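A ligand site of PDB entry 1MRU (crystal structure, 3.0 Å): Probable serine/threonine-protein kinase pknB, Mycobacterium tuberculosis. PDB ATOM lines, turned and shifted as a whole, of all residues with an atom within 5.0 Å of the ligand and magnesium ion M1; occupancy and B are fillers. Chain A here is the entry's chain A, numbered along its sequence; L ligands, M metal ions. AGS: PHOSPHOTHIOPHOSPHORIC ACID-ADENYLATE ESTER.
N of Ser 26 is in hydrogen-bond range of O1B of the ligand, 3.4 Å away.
The side-chain hydroxyl of Ser 26 sits at hydrogen-bond distance from an oxygen (O1B) of the ligand, at 2.5 Å.
The side-chain carboxylate (OD2) of Asp 159 lies within hydrogen-bond range of an oxygen (O2G) of the ligand, 2.6 Å away.
A nitrogen (N6) of the ligand is in hydrogen-bond range of the backbone carbonyl oxygen of Glu 96 (2.8 Å).
An oxygen (O1A) of the ligand is in salt-bridge range of the side-chain amino group of Lys 43, at 2.8 Å.
N1 of the ligand lies within hydrogen-bond range of N of Val 98, at 3.1 Å.
The backbone carbonyl oxygen of Leu 20 is in hydrogen-bond range of an oxygen (O2') of the ligand (3.5 Å).
OD1 of Asp 159 lies within salt-bridge range of NZ of Lys 43, 3.6 Å away.
OD2 of Asp 159 lies close to OD1 of Asn 146.
The backbone NH (N) of Gly 161 lies within hydrogen-bond range of the side-chain carboxylate (OD1) of Asp 159, at 3.4 Å.
The side-chain amino group (NZ) of Lys 43 is in salt-bridge range of the side-chain carboxylate (OE2) of Glu 62 (3.1 Å).
N of Leu 20 lies within hydrogen-bond range of O of Val 28 (3.0 Å).
The backbone carbonyl oxygen (O) of Asn 146 is in hydrogen-bond range of the backbone NH (N) of Met 158 (2.8 Å).
ND2 of Asn 146 is in hydrogen-bond range of O of Asp 141, at 2.9 Å.
N of Met 95 is in hydrogen-bond range of O of Ala 41.
Magnesium ion M1 is bound by O2B of the ligand (2.5 Å).
Slightly farther from magnesium ion M1 lies OD1 of Asp 159 (2.8 Å).
Slightly farther from magnesium ion M1 lies OD2 of Asp 159 (2.8 Å).
Merely in contact with magnesium ion M1: Gly 161.
CG2 of Val 28 touches O4' of the ligand, 3.6 Å away.
CB of Ala 41 touches N6 of the ligand, 3.6 Å away.
Val 75 touches the ligand.
Met 95 touches the ligand (SD to N7, 3.9 Å).
Tyr 97 touches the ligand.
CG2 of Thr 102 touches O3' of the ligand, at 3.3 Å.
Ala 145 touches the ligand (O to O3', 3.8 Å).
Asn 146 touches the ligand.
CE of Met 148 touches N3 of the ligand (3.6 Å).
Met 158 touches the ligand.
Hydrophobic or aromatic side chains that line the ligand: Leu 20, Val 28, Ala 41, Val 75, Met 95, Tyr 97, Val 98, Met 148 and Met 158.
Within 4 Å of the ligand: Leu 20, Ser 26, Val 28, Ala 41, Lys 43, Val 75, Met 95, Glu 96, Tyr 97, Val 98, Thr 102, Ala 145, Asn 146, Met 148, Met 158 and Asp 159.
The nearest printed residue that does not touch the ligand is Gly 23 (4.3 Å).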
ATOM      1  N   LEU A  20      23.709  -1.407 -14.011  1.00  0.00           N
ATOM      2  CA  LEU A  20      22.971  -2.646 -14.058  1.00  0.00           C
ATOM      3  C   LEU A  20      23.841  -3.797 -13.623  1.00  0.00           C
ATOM      4  O   LEU A  20      23.331  -4.840 -13.228  1.00  0.00           O
ATOM      5  CB  LEU A  20      22.443  -2.893 -15.467  1.00  0.00           C
ATOM      6  CG  LEU A  20      21.652  -1.719 -16.044  1.00  0.00           C
ATOM      7  CD1 LEU A  20      21.369  -2.010 -17.491  1.00  0.00           C
ATOM      8  CD2 LEU A  20      20.370  -1.465 -15.269  1.00  0.00           C
ATOM      9  N   GLY A  21      25.146  -3.602 -13.679  1.00  0.00           N
ATOM     10  CA  GLY A  21      26.034  -4.659 -13.257  1.00  0.00           C
ATOM     11  C   GLY A  21      27.487  -4.446 -13.618  1.00  0.00           C
ATOM     12  O   GLY A  21      27.777  -3.790 -14.606  1.00  0.00           O
ATOM     13  N   GLY A  23      30.994  -6.852 -13.804  1.00  0.00           N
ATOM     14  CA  GLY A  23      31.615  -8.141 -13.607  1.00  0.00           C
ATOM     15  C   GLY A  23      33.092  -8.108 -13.291  1.00  0.00           C
ATOM     16  O   GLY A  23      33.564  -7.327 -12.461  1.00  0.00           O
ATOM     17  N   GLY A  24      33.810  -8.999 -13.959  1.00  0.00           N
ATOM     18  CA  GLY A  24      35.243  -9.082 -13.796  1.00  0.00           C
ATOM     19  C   GLY A  24      35.893  -8.690 -15.122  1.00  0.00           C
ATOM     20  O   GLY A  24      37.092  -8.940 -15.348  1.00  0.00           O
ATOM     21  N   MET A  25      35.093  -8.075 -15.989  1.00  0.00           N
ATOM     22  CA  MET A  25      35.581  -7.633 -17.297  1.00  0.00           C
ATOM     23  C   MET A  25      34.956  -6.283 -17.657  1.00  0.00           C
ATOM     24  O   MET A  25      35.661  -5.375 -18.098  1.00  0.00           O
ATOM     25  CB  MET A  25      35.237  -8.663 -18.388  1.00  0.00           C
ATOM     26  CG  MET A  25      35.637  -8.224 -19.808  1.00  0.00           C
ATOM     27  SD  MET A  25      35.326  -9.449 -21.123  1.00  0.00           S
ATOM     28  CE  MET A  25      36.726  -9.051 -22.357  1.00  0.00           C
ATOM     29  N   SER A  26      33.652  -6.149 -17.479  1.00  0.00           N
ATOM     30  CA  SER A  26      33.012  -4.896 -17.803  1.00  0.00           C
ATOM     31  C   SER A  26      32.016  -4.436 -16.776  1.00  0.00           C
ATOM     32  O   SER A  26      31.739  -5.126 -15.795  1.00  0.00           O
ATOM     33  CB  SER A  26      32.338  -4.978 -19.175  1.00  0.00           C
ATOM     34  OG  SER A  26      31.358  -5.997 -19.201  1.00  0.00           O
ATOM     35  N   VAL A  28      28.206  -2.731 -16.991  1.00  0.00           N
ATOM     36  CA  VAL A  28      27.078  -2.379 -17.828  1.00  0.00           C
ATOM     37  C   VAL A  28      26.280  -1.284 -17.153  1.00  0.00           C
ATOM     38  O   VAL A  28      25.934  -1.393 -15.971  1.00  0.00           O
ATOM     39  CB  VAL A  28      26.184  -3.606 -18.058  1.00  0.00           C
ATOM     40  CG1 VAL A  28      25.084  -3.272 -19.038  1.00  0.00           C
ATOM     41  CG2 VAL A  28      27.029  -4.774 -18.561  1.00  0.00           C
ATOM     42  N   ALA A  41      21.360   0.168 -22.998  1.00  0.00           N
ATOM     43  CA  ALA A  41      22.261  -0.443 -22.022  1.00  0.00           C
ATOM     44  C   ALA A  41      23.647  -0.453 -22.658  1.00  0.00           C
ATOM     45  O   ALA A  41      23.854  -1.108 -23.670  1.00  0.00           O
ATOM     46  CB  ALA A  41      21.829  -1.861 -21.707  1.00  0.00           C
ATOM     47  N   LYS A  43      27.730  -1.256 -22.467  1.00  0.00           N
ATOM     48  CA  LYS A  43      28.713  -2.130 -21.825  1.00  0.00           C
ATOM     49  C   LYS A  43      30.059  -1.456 -22.007  1.00  0.00           C
ATOM     50  O   LYS A  43      30.440  -1.122 -23.126  1.00  0.00           O
ATOM     51  CB  LYS A  43      28.698  -3.486 -22.501  1.00  0.00           C
ATOM     52  CG  LYS A  43      29.504  -4.568 -21.816  1.00  0.00           C
ATOM     53  CD  LYS A  43      29.218  -5.910 -22.491  1.00  0.00           C
ATOM     54  CE  LYS A  43      29.747  -7.077 -21.704  1.00  0.00           C
ATOM     55  NZ  LYS A  43      29.292  -8.363 -22.302  1.00  0.00           N
ATOM     56  N   GLU A  62      33.216  -9.279 -29.849  1.00  0.00           N
ATOM     57  CA  GLU A  62      32.033  -9.780 -29.138  1.00  0.00           C
ATOM     58  C   GLU A  62      30.880  -8.876 -29.522  1.00  0.00           C
ATOM     59  O   GLU A  62      29.730  -9.308 -29.639  1.00  0.00           O
ATOM     60  CB  GLU A  62      32.204  -9.704 -27.637  1.00  0.00           C
ATOM     61  CG  GLU A  62      31.035 -10.290 -26.884  1.00  0.00           C
ATOM     62  CD  GLU A  62      30.764  -9.577 -25.578  1.00  0.00           C
ATOM     63  OE1 GLU A  62      31.745  -9.100 -24.956  1.00  0.00           O
ATOM     64  OE2 GLU A  62      29.573  -9.501 -25.170  1.00  0.00           O
ATOM     65  N   VAL A  75      19.677 -10.186 -27.303  1.00  0.00           N
ATOM     66  CA  VAL A  75      19.906  -8.758 -27.153  1.00  0.00           C
ATOM     67  C   VAL A  75      20.605  -8.204 -28.380  1.00  0.00           C
ATOM     68  O   VAL A  75      21.620  -8.714 -28.801  1.00  0.00           O
ATOM     69  CB  VAL A  75      20.772  -8.457 -25.924  1.00  0.00           C
ATOM     70  CG1 VAL A  75      21.036  -6.971 -25.823  1.00  0.00           C
ATOM     71  CG2 VAL A  75      20.076  -8.938 -24.673  1.00  0.00           C
ATOM     72  N   MET A  95      23.772  -1.714 -26.337  1.00  0.00           N
ATOM     73  CA  MET A  95      22.819  -2.795 -26.573  1.00  0.00           C
ATOM     74  C   MET A  95      21.399  -2.349 -26.283  1.00  0.00           C
ATOM     75  O   MET A  95      21.198  -1.262 -25.777  1.00  0.00           O
ATOM     76  CB  MET A  95      23.117  -3.982 -25.659  1.00  0.00           C
ATOM     77  CG  MET A  95      24.563  -4.404 -25.576  1.00  0.00           C
ATOM     78  SD  MET A  95      24.901  -5.212 -23.982  1.00  0.00           S
ATOM     79  CE  MET A  95      25.060  -6.963 -24.474  1.00  0.00           C
ATOM     80  N   GLU A  96      20.417  -3.199 -26.604  1.00  0.00           N
ATOM     81  CA  GLU A  96      19.021  -2.852 -26.299  1.00  0.00           C
ATOM     82  C   GLU A  96      18.932  -3.042 -24.796  1.00  0.00           C
ATOM     83  O   GLU A  96      19.611  -3.883 -24.225  1.00  0.00           O
ATOM     84  CB  GLU A  96      18.012  -3.779 -27.000  1.00  0.00           C
ATOM     85  CG  GLU A  96      17.947  -5.207 -26.480  1.00  0.00           C
ATOM     86  CD  GLU A  96      16.825  -6.019 -27.112  1.00  0.00           C
ATOM     87  OE1 GLU A  96      15.640  -5.764 -26.788  1.00  0.00           O
ATOM     88  OE2 GLU A  96      17.107  -6.936 -27.925  1.00  0.00           O
ATOM     89  N   TYR A  97      18.099  -2.242 -24.139  1.00  0.00           N
ATOM     90  CA  TYR A  97      17.969  -2.348 -22.702  1.00  0.00           C
ATOM     91  C   TYR A  97      16.895  -3.335 -22.303  1.00  0.00           C
ATOM     92  O   TYR A  97      15.775  -3.278 -22.810  1.00  0.00           O
ATOM     93  CB  TYR A  97      17.671  -0.974 -22.110  1.00  0.00           C
ATOM     94  CG  TYR A  97      17.271  -0.998 -20.665  1.00  0.00           C
ATOM     95  CD1 TYR A  97      18.092  -1.578 -19.702  1.00  0.00           C
ATOM     96  CD2 TYR A  97      16.053  -0.450 -20.259  1.00  0.00           C
ATOM     97  CE1 TYR A  97      17.704  -1.600 -18.366  1.00  0.00           C
ATOM     98  CE2 TYR A  97      15.651  -0.472 -18.922  1.00  0.00           C
ATOM     99  CZ  TYR A  97      16.482  -1.049 -17.984  1.00  0.00           C
ATOM    100  OH  TYR A  97      16.090  -1.069 -16.673  1.00  0.00           O
ATOM    101  N   VAL A  98      17.252  -4.242 -21.401  1.00  0.00           N
ATOM    102  CA  VAL A  98      16.319  -5.246 -20.916  1.00  0.00           C
ATOM    103  C   VAL A  98      16.070  -5.012 -19.450  1.00  0.00           C
ATOM    104  O   VAL A  98      16.862  -5.442 -18.618  1.00  0.00           O
ATOM    105  CB  VAL A  98      16.857  -6.676 -21.052  1.00  0.00           C
ATOM    106  CG1 VAL A  98      15.823  -7.644 -20.573  1.00  0.00           C
ATOM    107  CG2 VAL A  98      17.258  -6.976 -22.466  1.00  0.00           C
ATOM    108  N   THR A 102      18.400 -11.877 -14.620  1.00  0.00           N
ATOM    109  CA  THR A 102      18.993 -13.059 -15.233  1.00  0.00           C
ATOM    110  C   THR A 102      18.320 -14.217 -14.548  1.00  0.00           C
ATOM    111  O   THR A 102      17.710 -14.030 -13.491  1.00  0.00           O
ATOM    112  CB  THR A 102      20.501 -13.213 -14.957  1.00  0.00           C
ATOM    113  OG1 THR A 102      20.720 -13.406 -13.546  1.00  0.00           O
ATOM    114  CG2 THR A 102      21.259 -12.009 -15.450  1.00  0.00           C
ATOM    115  N   ASP A 141      29.008 -19.972 -24.061  1.00  0.00           N
ATOM    116  CA  ASP A 141      28.787 -19.571 -22.679  1.00  0.00           C
ATOM    117  C   ASP A 141      27.311 -19.477 -22.305  1.00  0.00           C
ATOM    118  O   ASP A 141      26.825 -18.405 -21.946  1.00  0.00           O
ATOM    119  CB  ASP A 141      29.507 -18.243 -22.452  1.00  0.00           C
ATOM    120  CG  ASP A 141      29.598 -17.836 -20.991  1.00  0.00           C
ATOM    121  OD1 ASP A 141      29.822 -18.697 -20.122  1.00  0.00           O
ATOM    122  OD2 ASP A 141      29.447 -16.623 -20.719  1.00  0.00           O
ATOM    123  N   ALA A 145      22.976 -17.189 -15.950  1.00  0.00           N
ATOM    124  CA  ALA A 145      23.258 -15.775 -15.781  1.00  0.00           C
ATOM    125  C   ALA A 145      23.267 -15.024 -17.114  1.00  0.00           C
ATOM    126  O   ALA A 145      23.382 -13.791 -17.124  1.00  0.00           O
ATOM    127  CB  ALA A 145      24.585 -15.597 -15.064  1.00  0.00           C
ATOM    128  N   ASN A 146      23.167 -15.751 -18.225  1.00  0.00           N
ATOM    129  CA  ASN A 146      23.175 -15.097 -19.524  1.00  0.00           C
ATOM    130  C   ASN A 146      21.847 -15.124 -20.239  1.00  0.00           C
ATOM    131  O   ASN A 146      21.763 -14.780 -21.411  1.00  0.00           O
ATOM    132  CB  ASN A 146      24.265 -15.673 -20.413  1.00  0.00           C
ATOM    133  CG  ASN A 146      25.649 -15.260 -19.967  1.00  0.00           C
ATOM    134  OD1 ASN A 146      25.841 -14.152 -19.464  1.00  0.00           O
ATOM    135  ND2 ASN A 146      26.617 -16.146 -20.152  1.00  0.00           N
ATOM    136  N   MET A 148      18.044 -13.614 -19.747  1.00  0.00           N
ATOM    137  CA  MET A 148      17.286 -12.655 -18.958  1.00  0.00           C
ATOM    138  C   MET A 148      15.793 -12.818 -19.157  1.00  0.00           C
ATOM    139  O   MET A 148      15.332 -13.298 -20.177  1.00  0.00           O
ATOM    140  CB  MET A 148      17.700 -11.211 -19.299  1.00  0.00           C
ATOM    141  CG  MET A 148      18.976 -10.732 -18.613  1.00  0.00           C
ATOM    142  SD  MET A 148      19.412  -8.977 -18.879  1.00  0.00           S
ATOM    143  CE  MET A 148      18.869  -8.232 -17.379  1.00  0.00           C
ATOM    144  N   MET A 158      21.972 -13.115 -23.645  1.00  0.00           N
ATOM    145  CA  MET A 158      22.893 -11.991 -23.814  1.00  0.00           C
ATOM    146  C   MET A 158      24.422 -12.030 -23.777  1.00  0.00           C
ATOM    147  O   MET A 158      25.035 -11.013 -24.104  1.00  0.00           O
ATOM    148  CB  MET A 158      22.454 -10.900 -22.844  1.00  0.00           C
ATOM    149  CG  MET A 158      21.996 -11.441 -21.536  1.00  0.00           C
ATOM    150  SD  MET A 158      22.243 -10.291 -20.225  1.00  0.00           S
ATOM    151  CE  MET A 158      23.706 -10.973 -19.470  1.00  0.00           C
ATOM    152  N   ASP A 159      25.087 -13.118 -23.417  1.00  0.00           N
ATOM    153  CA  ASP A 159      26.532 -12.986 -23.401  1.00  0.00           C
ATOM    154  C   ASP A 159      27.274 -13.678 -24.518  1.00  0.00           C
ATOM    155  O   ASP A 159      27.186 -14.875 -24.669  1.00  0.00           O
ATOM    156  CB  ASP A 159      27.101 -13.412 -22.053  1.00  0.00           C
ATOM    157  CG  ASP A 159      28.297 -12.574 -21.641  1.00  0.00           C
ATOM    158  OD1 ASP A 159      28.829 -11.896 -22.537  1.00  0.00           O
ATOM    159  OD2 ASP A 159      28.709 -12.608 -20.455  1.00  0.00           O
ATOM    160  N   GLY A 161      30.737 -12.813 -25.160  1.00  0.00           N
ATOM    161  CA  GLY A 161      32.155 -12.577 -24.936  1.00  0.00           C
ATOM    162  C   GLY A 161      33.068 -13.776 -25.179  1.00  0.00           C
ATOM    163  O   GLY A 161      34.260 -13.593 -25.418  1.00  0.00           O
ATOM    164  N   ILE A 162      32.516 -14.976 -25.124  1.00  0.00           N
ATOM    165  CA  ILE A 162      33.286 -16.208 -25.321  1.00  0.00           C
ATOM    166  C   ILE A 162      32.711 -16.994 -26.505  1.00  0.00           C
ATOM    167  O   ILE A 162      32.960 -18.194 -26.645  1.00  0.00           O
ATOM    168  CB  ILE A 162      33.269 -17.069 -24.004  1.00  0.00           C
ATOM    169  CG1 ILE A 162      34.243 -16.465 -22.980  1.00  0.00           C
ATOM    170  CG2 ILE A 162      33.674 -18.506 -24.262  1.00  0.00           C
ATOM    171  CD1 ILE A 162      33.918 -15.023 -22.567  1.00  0.00           C
HETATM  172  PG  AGS L   1      30.863 -11.945 -17.164  1.00  0.00           P
HETATM  173  S1G AGS L   1      30.971 -12.908 -15.388  1.00  0.00           S
HETATM  174  O2G AGS L   1      29.665 -12.598 -18.007  1.00  0.00           O
HETATM  175  O3G AGS L   1      32.194 -12.102 -17.885  1.00  0.00           O
HETATM  176  PB  AGS L   1      30.198  -9.388 -18.242  1.00  0.00           P
HETATM  177  O1B AGS L   1      30.975  -8.158 -18.073  1.00  0.00           O
HETATM  178  O2B AGS L   1      30.409 -10.237 -19.527  1.00  0.00           O
HETATM  179  O3B AGS L   1      30.439 -10.401 -17.023  1.00  0.00           O
HETATM  180  PA  AGS L   1      27.442  -9.539 -18.804  1.00  0.00           P
HETATM  181  O1A AGS L   1      27.418  -9.014 -20.284  1.00  0.00           O
HETATM  182  O2A AGS L   1      27.391 -11.065 -18.826  1.00  0.00           O
HETATM  183  O3A AGS L   1      28.686  -9.091 -18.005  1.00  0.00           O
HETATM  184  O5' AGS L   1      26.271  -8.803 -17.975  1.00  0.00           O
HETATM  185  C5' AGS L   1      26.461  -8.391 -16.566  1.00  0.00           C
HETATM  186  C4' AGS L   1      25.085  -8.002 -16.035  1.00  0.00           C
HETATM  187  O4' AGS L   1      24.748  -6.801 -16.726  1.00  0.00           O
HETATM  188  C3' AGS L   1      23.997  -8.957 -16.448  1.00  0.00           C
HETATM  189  O3' AGS L   1      24.034 -10.277 -15.806  1.00  0.00           O
HETATM  190  C2' AGS L   1      22.841  -7.952 -16.317  1.00  0.00           C
HETATM  191  O2' AGS L   1      22.400  -7.678 -14.976  1.00  0.00           O
HETATM  192  C1' AGS L   1      23.408  -6.725 -16.936  1.00  0.00           C
HETATM  193  N9  AGS L   1      23.163  -6.580 -18.387  1.00  0.00           N
HETATM  194  C8  AGS L   1      23.907  -6.939 -19.473  1.00  0.00           C
HETATM  195  N7  AGS L   1      23.345  -6.610 -20.638  1.00  0.00           N
HETATM  196  C5  AGS L   1      22.165  -6.007 -20.256  1.00  0.00           C
HETATM  197  C6  AGS L   1      21.110  -5.414 -21.021  1.00  0.00           C
HETATM  198  N6  AGS L   1      21.026  -5.331 -22.253  1.00  0.00           N
HETATM  199  N1  AGS L   1      20.098  -4.913 -20.240  1.00  0.00           N
HETATM  200  C2  AGS L   1      20.068  -4.938 -18.854  1.00  0.00           C
HETATM  201  N3  AGS L   1      21.032  -5.467 -18.126  1.00  0.00           N
HETATM  202  C4  AGS L   1      22.054  -5.984 -18.882  1.00  0.00           C
HETATM  203 MG    MG M   1      31.308 -11.818 -21.289  1.00  0.00          MG
HETATM  204 MG    MG M   2      26.716 -12.311 -16.177  1.00  0.00          MG
